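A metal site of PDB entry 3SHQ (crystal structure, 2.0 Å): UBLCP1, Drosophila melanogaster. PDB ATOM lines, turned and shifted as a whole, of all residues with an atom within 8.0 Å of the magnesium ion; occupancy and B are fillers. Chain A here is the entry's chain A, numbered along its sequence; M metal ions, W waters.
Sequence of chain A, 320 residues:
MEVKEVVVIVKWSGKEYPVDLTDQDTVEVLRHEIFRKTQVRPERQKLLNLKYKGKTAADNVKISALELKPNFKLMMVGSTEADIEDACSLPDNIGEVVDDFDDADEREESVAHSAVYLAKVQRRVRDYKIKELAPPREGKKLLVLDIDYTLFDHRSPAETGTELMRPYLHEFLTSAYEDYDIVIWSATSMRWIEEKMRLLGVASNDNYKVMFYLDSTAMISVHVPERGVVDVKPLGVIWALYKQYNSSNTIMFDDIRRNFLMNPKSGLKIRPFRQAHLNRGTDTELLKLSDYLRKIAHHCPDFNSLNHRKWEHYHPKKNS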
ATOM      1  N   GLY A  95     -18.833  27.472  -2.055  1.00  0.00           N
ATOM      2  CA  GLY A  95     -19.329  27.632  -3.413  1.00  0.00           C
ATOM      3  C   GLY A  95     -18.878  28.939  -4.042  1.00  0.00           C
ATOM      4  O   GLY A  95     -17.875  29.534  -3.618  1.00  0.00           O
ATOM      5  N   GLU A  96     -19.620  29.387  -5.041  1.00  0.00           N
ATOM      6  CA  GLU A  96     -19.295  30.617  -5.757  1.00  0.00           C
ATOM      7  C   GLU A  96     -20.560  31.425  -6.006  1.00  0.00           C
ATOM      8  O   GLU A  96     -21.663  30.873  -6.056  1.00  0.00           O
ATOM      9  CB  GLU A  96     -18.614  30.303  -7.091  1.00  0.00           C
ATOM     10  CG  GLU A  96     -17.325  29.510  -6.949  1.00  0.00           C
ATOM     11  CD  GLU A  96     -16.477  29.540  -8.202  1.00  0.00           C
ATOM     12  OE1 GLU A  96     -17.037  29.659  -9.318  1.00  0.00           O
ATOM     13  OE2 GLU A  96     -15.232  29.457  -8.070  1.00  0.00           O
ATOM     14  N   VAL A  97     -20.411  32.737  -6.174  1.00  0.00           N
ATOM     15  CA  VAL A  97     -21.586  33.589  -6.391  1.00  0.00           C
ATOM     16  C   VAL A  97     -21.514  34.375  -7.688  1.00  0.00           C
ATOM     17  O   VAL A  97     -22.521  34.868  -8.193  1.00  0.00           O
ATOM     18  CB  VAL A  97     -21.806  34.560  -5.207  1.00  0.00           C
ATOM     19  CG1 VAL A  97     -22.209  33.776  -3.957  1.00  0.00           C
ATOM     20  CG2 VAL A  97     -20.559  35.384  -4.953  1.00  0.00           C
ATOM     21  N   VAL A  98     -20.315  34.498  -8.256  1.00  0.00           N
ATOM     22  CA  VAL A  98     -20.161  35.291  -9.472  1.00  0.00           C
ATOM     23  C   VAL A  98     -18.807  35.037 -10.112  1.00  0.00           C
ATOM     24  O   VAL A  98     -17.860  34.632  -9.431  1.00  0.00           O
ATOM     25  CB  VAL A  98     -20.291  36.810  -9.156  1.00  0.00           C
ATOM     26  CG1 VAL A  98     -19.039  37.311  -8.407  1.00  0.00           C
ATOM     27  CG2 VAL A  98     -20.538  37.620 -10.429  1.00  0.00           C
ATOM     28  N   LEU A 145     -26.558  19.382 -13.926  1.00  0.00           N
ATOM     29  CA  LEU A 145     -27.026  20.536 -13.174  1.00  0.00           C
ATOM     30  C   LEU A 145     -26.056  20.957 -12.091  1.00  0.00           C
ATOM     31  O   LEU A 145     -25.652  20.160 -11.230  1.00  0.00           O
ATOM     32  CB  LEU A 145     -28.368  20.215 -12.496  1.00  0.00           C
ATOM     33  CG  LEU A 145     -29.560  19.952 -13.430  1.00  0.00           C
ATOM     34  CD1 LEU A 145     -30.721  19.465 -12.588  1.00  0.00           C
ATOM     35  CD2 LEU A 145     -29.922  21.222 -14.216  1.00  0.00           C
ATOM     36  N   ASP A 146     -25.706  22.241 -12.118  1.00  0.00           N
ATOM     37  CA  ASP A 146     -25.054  22.873 -10.985  1.00  0.00           C
ATOM     38  C   ASP A 146     -26.020  22.962  -9.809  1.00  0.00           C
ATOM     39  O   ASP A 146     -27.241  22.804  -9.980  1.00  0.00           O
ATOM     40  CB  ASP A 146     -24.612  24.276 -11.421  1.00  0.00           C
ATOM     41  CG  ASP A 146     -23.970  25.051 -10.311  1.00  0.00           C
ATOM     42  OD1 ASP A 146     -23.020  24.539  -9.689  1.00  0.00           O
ATOM     43  OD2 ASP A 146     -24.429  26.179 -10.067  1.00  0.00           O
ATOM     44  N   ILE A 147     -25.500  23.195  -8.597  1.00  0.00           N
ATOM     45  CA  ILE A 147     -26.357  23.439  -7.445  1.00  0.00           C
ATOM     46  C   ILE A 147     -26.420  24.920  -7.021  1.00  0.00           C
ATOM     47  O   ILE A 147     -27.501  25.520  -7.017  1.00  0.00           O
ATOM     48  CB  ILE A 147     -25.946  22.622  -6.205  1.00  0.00           C
ATOM     49  CG1 ILE A 147     -25.827  21.125  -6.537  1.00  0.00           C
ATOM     50  CG2 ILE A 147     -26.974  22.818  -5.101  1.00  0.00           C
ATOM     51  CD1 ILE A 147     -25.331  20.272  -5.347  1.00  0.00           C
ATOM     52  N   ASP A 148     -25.280  25.486  -6.631  1.00  0.00           N
ATOM     53  CA  ASP A 148     -25.315  26.834  -6.025  1.00  0.00           C
ATOM     54  C   ASP A 148     -25.785  27.934  -6.967  1.00  0.00           C
ATOM     55  O   ASP A 148     -25.214  28.130  -8.024  1.00  0.00           O
ATOM     56  CB  ASP A 148     -24.002  27.214  -5.280  1.00  0.00           C
ATOM     57  CG  ASP A 148     -22.742  27.103  -6.126  1.00  0.00           C
ATOM     58  OD1 ASP A 148     -22.772  26.742  -7.328  1.00  0.00           O
ATOM     59  OD2 ASP A 148     -21.657  27.406  -5.579  1.00  0.00           O
ATOM     60  N   TYR A 149     -26.842  28.633  -6.556  1.00  0.00           N
ATOM     61  CA  TYR A 149     -27.490  29.666  -7.354  1.00  0.00           C
ATOM     62  C   TYR A 149     -28.187  29.101  -8.591  1.00  0.00           C
ATOM     63  O   TYR A 149     -28.805  29.839  -9.371  1.00  0.00           O
ATOM     64  CB  TYR A 149     -26.533  30.781  -7.750  1.00  0.00           C
ATOM     65  CG  TYR A 149     -26.350  31.889  -6.726  1.00  0.00           C
ATOM     66  CD1 TYR A 149     -25.521  32.965  -6.988  1.00  0.00           C
ATOM     67  CD2 TYR A 149     -27.019  31.872  -5.499  1.00  0.00           C
ATOM     68  CE1 TYR A 149     -25.341  33.996  -6.085  1.00  0.00           C
ATOM     69  CE2 TYR A 149     -26.852  32.893  -4.556  1.00  0.00           C
ATOM     70  CZ  TYR A 149     -26.006  33.960  -4.869  1.00  0.00           C
ATOM     71  OH  TYR A 149     -25.819  35.002  -3.980  1.00  0.00           O
ATOM     72  N   THR A 150     -28.081  27.784  -8.792  1.00  0.00           N
ATOM     73  CA  THR A 150     -28.775  27.152  -9.905  1.00  0.00           C
ATOM     74  C   THR A 150     -30.088  26.524  -9.441  1.00  0.00           C
ATOM     75  O   THR A 150     -31.156  26.845  -9.989  1.00  0.00           O
ATOM     76  CB  THR A 150     -27.856  26.129 -10.617  1.00  0.00           C
ATOM     77  OG1 THR A 150     -26.781  26.832 -11.257  1.00  0.00           O
ATOM     78  CG2 THR A 150     -28.631  25.313 -11.675  1.00  0.00           C
ATOM     79  N   LEU A 151     -30.025  25.673  -8.412  1.00  0.00           N
ATOM     80  CA  LEU A 151     -31.207  25.014  -7.869  1.00  0.00           C
ATOM     81  C   LEU A 151     -31.620  25.601  -6.520  1.00  0.00           C
ATOM     82  O   LEU A 151     -32.699  25.305  -6.017  1.00  0.00           O
ATOM     83  CB  LEU A 151     -30.937  23.530  -7.679  1.00  0.00           C
ATOM     84  CG  LEU A 151     -30.442  22.815  -8.934  1.00  0.00           C
ATOM     85  CD1 LEU A 151     -30.163  21.351  -8.595  1.00  0.00           C
ATOM     86  CD2 LEU A 151     -31.471  22.935 -10.060  1.00  0.00           C
ATOM     87  N   PHE A 152     -30.767  26.427  -5.928  1.00  0.00           N
ATOM     88  CA  PHE A 152     -31.129  27.027  -4.651  1.00  0.00           C
ATOM     89  C   PHE A 152     -30.220  28.177  -4.237  1.00  0.00           C
ATOM     90  O   PHE A 152     -29.161  28.387  -4.836  1.00  0.00           O
ATOM     91  CB  PHE A 152     -31.229  25.962  -3.546  1.00  0.00           C
ATOM     92  CG  PHE A 152     -29.974  25.782  -2.735  1.00  0.00           C
ATOM     93  CD1 PHE A 152     -28.776  25.424  -3.338  1.00  0.00           C
ATOM     94  CD2 PHE A 152     -29.999  25.940  -1.359  1.00  0.00           C
ATOM     95  CE1 PHE A 152     -27.628  25.249  -2.585  1.00  0.00           C
ATOM     96  CE2 PHE A 152     -28.849  25.776  -0.598  1.00  0.00           C
ATOM     97  CZ  PHE A 152     -27.664  25.422  -1.205  1.00  0.00           C
ATOM     98  N   HIS A 154     -27.744  29.478  -1.855  1.00  0.00           N
ATOM     99  CA  HIS A 154     -26.809  28.958  -0.867  1.00  0.00           C
ATOM    100  C   HIS A 154     -26.220  30.051   0.035  1.00  0.00           C
ATOM    101  O   HIS A 154     -25.347  29.777   0.850  1.00  0.00           O
ATOM    102  CB  HIS A 154     -25.669  28.211  -1.559  1.00  0.00           C
ATOM    103  CG  HIS A 154     -24.836  29.081  -2.457  1.00  0.00           C
ATOM    104  ND1 HIS A 154     -25.385  29.833  -3.468  1.00  0.00           N
ATOM    105  CD2 HIS A 154     -23.507  29.325  -2.490  1.00  0.00           C
ATOM    106  CE1 HIS A 154     -24.424  30.499  -4.097  1.00  0.00           C
ATOM    107  NE2 HIS A 154     -23.272  30.205  -3.516  1.00  0.00           N
ATOM    108  N   TRP A 185     -23.608  18.260 -10.671  1.00  0.00           N
ATOM    109  CA  TRP A 185     -22.173  18.552 -10.608  1.00  0.00           C
ATOM    110  C   TRP A 185     -21.914  19.883  -9.916  1.00  0.00           C
ATOM    111  O   TRP A 185     -22.157  20.949 -10.488  1.00  0.00           O
ATOM    112  CB  TRP A 185     -21.567  18.578 -12.002  1.00  0.00           C
ATOM    113  CG  TRP A 185     -20.061  18.409 -11.991  1.00  0.00           C
ATOM    114  CD1 TRP A 185     -19.212  18.571 -10.910  1.00  0.00           C
ATOM    115  CD2 TRP A 185     -19.231  18.007 -13.083  1.00  0.00           C
ATOM    116  NE1 TRP A 185     -17.922  18.294 -11.284  1.00  0.00           N
ATOM    117  CE2 TRP A 185     -17.907  17.955 -12.606  1.00  0.00           C
ATOM    118  CE3 TRP A 185     -19.497  17.684 -14.422  1.00  0.00           C
ATOM    119  CZ2 TRP A 185     -16.841  17.588 -13.433  1.00  0.00           C
ATOM    120  CZ3 TRP A 185     -18.433  17.322 -15.233  1.00  0.00           C
ATOM    121  CH2 TRP A 185     -17.117  17.284 -14.737  1.00  0.00           C
ATOM    122  N   SER A 186     -21.416  19.796  -8.689  1.00  0.00           N
ATOM    123  CA  SER A 186     -21.184  20.958  -7.826  1.00  0.00           C
ATOM    124  C   SER A 186     -19.687  21.130  -7.583  1.00  0.00           C
ATOM    125  O   SER A 186     -18.972  20.143  -7.374  1.00  0.00           O
ATOM    126  CB  SER A 186     -21.905  20.722  -6.489  1.00  0.00           C
ATOM    127  OG  SER A 186     -21.601  21.742  -5.547  1.00  0.00           O
ATOM    128  N   ALA A 187     -19.205  22.370  -7.645  1.00  0.00           N
ATOM    129  CA  ALA A 187     -17.790  22.663  -7.369  1.00  0.00           C
ATOM    130  C   ALA A 187     -17.533  22.703  -5.866  1.00  0.00           C
ATOM    131  O   ALA A 187     -16.996  23.679  -5.343  1.00  0.00           O
ATOM    132  CB  ALA A 187     -17.374  24.007  -8.028  1.00  0.00           C
ATOM    133  N   TRP A 192     -20.975  18.059   0.908  1.00  0.00           N
ATOM    134  CA  TRP A 192     -21.834  19.232   0.787  1.00  0.00           C
ATOM    135  C   TRP A 192     -22.995  18.925  -0.176  1.00  0.00           C
ATOM    136  O   TRP A 192     -24.153  19.257   0.102  1.00  0.00           O
ATOM    137  CB  TRP A 192     -21.026  20.434   0.303  1.00  0.00           C
ATOM    138  CG  TRP A 192     -21.734  21.763   0.361  1.00  0.00           C
ATOM    139  CD1 TRP A 192     -21.755  22.625   1.431  1.00  0.00           C
ATOM    140  CD2 TRP A 192     -22.482  22.391  -0.685  1.00  0.00           C
ATOM    141  NE1 TRP A 192     -22.491  23.751   1.114  1.00  0.00           N
ATOM    142  CE2 TRP A 192     -22.948  23.629  -0.174  1.00  0.00           C
ATOM    143  CE3 TRP A 192     -22.822  22.029  -1.995  1.00  0.00           C
ATOM    144  CZ2 TRP A 192     -23.732  24.508  -0.933  1.00  0.00           C
ATOM    145  CZ3 TRP A 192     -23.603  22.894  -2.748  1.00  0.00           C
ATOM    146  CH2 TRP A 192     -24.039  24.122  -2.217  1.00  0.00           C
ATOM    147  N   LYS A 233     -15.715  22.303 -15.254  1.00  0.00           N
ATOM    148  CA  LYS A 233     -16.397  21.019 -15.120  1.00  0.00           C
ATOM    149  C   LYS A 233     -16.423  20.369 -16.496  1.00  0.00           C
ATOM    150  O   LYS A 233     -17.273  20.679 -17.328  1.00  0.00           O
ATOM    151  CB  LYS A 233     -17.820  21.209 -14.596  1.00  0.00           C
ATOM    152  CG  LYS A 233     -17.895  21.841 -13.202  1.00  0.00           C
ATOM    153  CD  LYS A 233     -19.320  22.232 -12.812  1.00  0.00           C
ATOM    154  CE  LYS A 233     -19.331  23.036 -11.516  1.00  0.00           C
ATOM    155  NZ  LYS A 233     -20.698  23.429 -11.046  1.00  0.00           N
ATOM    156  N   PHE A 253     -26.692  23.095 -17.094  1.00  0.00           N
ATOM    157  CA  PHE A 253     -27.119  24.380 -16.558  1.00  0.00           C
ATOM    158  C   PHE A 253     -26.148  24.769 -15.457  1.00  0.00           C
ATOM    159  O   PHE A 253     -25.893  23.974 -14.548  1.00  0.00           O
ATOM    160  CB  PHE A 253     -28.509  24.293 -15.909  1.00  0.00           C
ATOM    161  CG  PHE A 253     -29.660  24.110 -16.873  1.00  0.00           C
ATOM    162  CD1 PHE A 253     -29.448  24.040 -18.243  1.00  0.00           C
ATOM    163  CD2 PHE A 253     -30.964  24.042 -16.394  1.00  0.00           C
ATOM    164  CE1 PHE A 253     -30.509  23.885 -19.132  1.00  0.00           C
ATOM    165  CE2 PHE A 253     -32.049  23.883 -17.283  1.00  0.00           C
ATOM    166  CZ  PHE A 253     -31.808  23.809 -18.655  1.00  0.00           C
ATOM    167  N   ASP A 254     -25.599  25.982 -15.520  1.00  0.00           N
ATOM    168  CA  ASP A 254     -24.711  26.466 -14.457  1.00  0.00           C
ATOM    169  C   ASP A 254     -24.815  27.986 -14.467  1.00  0.00           C
ATOM    170  O   ASP A 254     -24.966  28.588 -15.528  1.00  0.00           O
ATOM    171  CB  ASP A 254     -23.277  25.976 -14.729  1.00  0.00           C
ATOM    172  CG  ASP A 254     -22.379  26.006 -13.495  1.00  0.00           C
ATOM    173  OD1 ASP A 254     -22.294  27.060 -12.828  1.00  0.00           O
ATOM    174  OD2 ASP A 254     -21.735  24.976 -13.206  1.00  0.00           O
ATOM    175  N   ASP A 255     -24.758  28.625 -13.294  1.00  0.00           N
ATOM    176  CA  ASP A 255     -24.813  30.088 -13.295  1.00  0.00           C
ATOM    177  C   ASP A 255     -23.446  30.691 -13.608  1.00  0.00           C
ATOM    178  O   ASP A 255     -23.325  31.885 -13.909  1.00  0.00           O
ATOM    179  CB  ASP A 255     -25.328  30.640 -11.952  1.00  0.00           C
ATOM    180  CG  ASP A 255     -24.443  30.243 -10.786  1.00  0.00           C
ATOM    181  OD1 ASP A 255     -23.953  31.138 -10.054  1.00  0.00           O
ATOM    182  OD2 ASP A 255     -24.235  29.038 -10.600  1.00  0.00           O
ATOM    183  N   ILE A 256     -22.410  29.854 -13.550  1.00  0.00           N
ATOM    184  CA  ILE A 256     -21.057  30.354 -13.784  1.00  0.00           C
ATOM    185  C   ILE A 256     -20.559  29.825 -15.119  1.00  0.00           C
ATOM    186  O   ILE A 256     -20.216  28.654 -15.225  1.00  0.00           O
ATOM    187  CB  ILE A 256     -20.099  29.954 -12.639  1.00  0.00           C
ATOM    188  CG1 ILE A 256     -20.597  30.507 -11.301  1.00  0.00           C
ATOM    189  CG2 ILE A 256     -18.671  30.428 -12.934  1.00  0.00           C
ATOM    190  CD1 ILE A 256     -20.631  32.033 -11.248  1.00  0.00           C
ATOM    191  N   ASN A 259     -17.475  27.452 -15.889  1.00  0.00           N
ATOM    192  CA  ASN A 259     -17.532  26.013 -15.676  1.00  0.00           C
ATOM    193  C   ASN A 259     -17.604  25.186 -16.974  1.00  0.00           C
ATOM    194  O   ASN A 259     -17.122  24.053 -17.002  1.00  0.00           O
ATOM    195  CB  ASN A 259     -18.648  25.645 -14.705  1.00  0.00           C
ATOM    196  CG  ASN A 259     -18.289  25.977 -13.265  1.00  0.00           C
ATOM    197  OD1 ASN A 259     -19.112  26.484 -12.502  1.00  0.00           O
ATOM    198  ND2 ASN A 259     -17.038  25.730 -12.906  1.00  0.00           N
ATOM    199  N   ILE A 270     -27.533  29.863 -16.581  1.00  0.00           N
ATOM    200  CA  ILE A 270     -28.814  30.149 -15.950  1.00  0.00           C
ATOM    201  C   ILE A 270     -28.706  31.431 -15.141  1.00  0.00           C
ATOM    202  O   ILE A 270     -27.630  31.750 -14.626  1.00  0.00           O
ATOM    203  CB  ILE A 270     -29.259  28.971 -15.046  1.00  0.00           C
ATOM    204  CG1 ILE A 270     -30.728  29.119 -14.611  1.00  0.00           C
ATOM    205  CG2 ILE A 270     -28.332  28.801 -13.846  1.00  0.00           C
ATOM    206  CD1 ILE A 270     -31.311  27.829 -13.979  1.00  0.00           C
ATOM    207  N   PRO A 272     -28.818  33.477 -11.909  1.00  0.00           N
ATOM    208  CA  PRO A 272     -28.626  32.981 -10.535  1.00  0.00           C
ATOM    209  C   PRO A 272     -29.832  33.238  -9.654  1.00  0.00           C
ATOM    210  O   PRO A 272     -30.440  34.308  -9.755  1.00  0.00           O
ATOM    211  CB  PRO A 272     -27.421  33.782 -10.043  1.00  0.00           C
ATOM    212  CG  PRO A 272     -27.452  35.047 -10.848  1.00  0.00           C
ATOM    213  CD  PRO A 272     -27.938  34.618 -12.207  1.00  0.00           C
HETATM  214 MG    MG M   1     -23.399  27.766  -9.073  1.00  0.00          MG
HETATM  215  O   HOH W   1     -22.615  29.619  -8.374  1.00  0.00           O
HETATM  216  O   HOH W   2     -21.757  27.487 -10.144  1.00  0.00           O
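Asp 254 touches the magnesium ion (OD1 to MG, 3.98 Å). Of the 25 residues printed, 4 come within 4 Å of the magnesium ion. The nearest printed residue that does not touch the magnesium ion is Thr 150 (4.1 Å).
Water W1 bridges OD1 of Asp 255 and O of Glu 96. Water W2 bridges the side-chain carboxylate (OD1) of Asp 254 (2.8 Å) and the side-chain carboxylate (OD1) of Asp 146 (3.2 Å).
The magnesium ion is bound by water W2 (2.0 Å), the side-chain carboxylate (OD1) of Asp 148 (2.1 Å), the backbone carbonyl oxygen (O) of Asp 148 (2.1 Å), water W1 (2.1 Å), the side-chain carboxylate (OD2) of Asp 146 (2.1 Å) and the side-chain carboxylate (OD2) of Asp 255 (2.2 Å).
The side-chain carboxylate (OD2) of Asp 148 is in hydrogen-bond range of the backbone NH (N) of Glu 96 (2.9 Å). OD2 of Asp 146 sits close to OG1 of Thr 150, at 2.7 Å. N of Ile 270 is in hydrogen-bond range of O of Asp 254, at 3.1 Å. The backbone NH (N) of Ile 256 sits at hydrogen-bond distance from the side-chain carboxylate (OD1) of Asp 254 (2.9 Å). The side-chain amino group (NZ) of Lys 233 lies within salt-bridge range of the side-chain carboxylate (OD1) of Asp 146, at 2.9 Å. The side-chain hydroxyl (OG1) of Thr 150 is in hydrogen-bond range of the backbone NH (N) of Asp 255 (3.4 Å). OD2 of Asp 254 lies close to OD1 of Asn 259 (3.1 Å). The backbone carbonyl oxygen (O) of Phe 253 is in hydrogen-bond range of the backbone NH (N) of Asp 146, at 3.0 Å.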
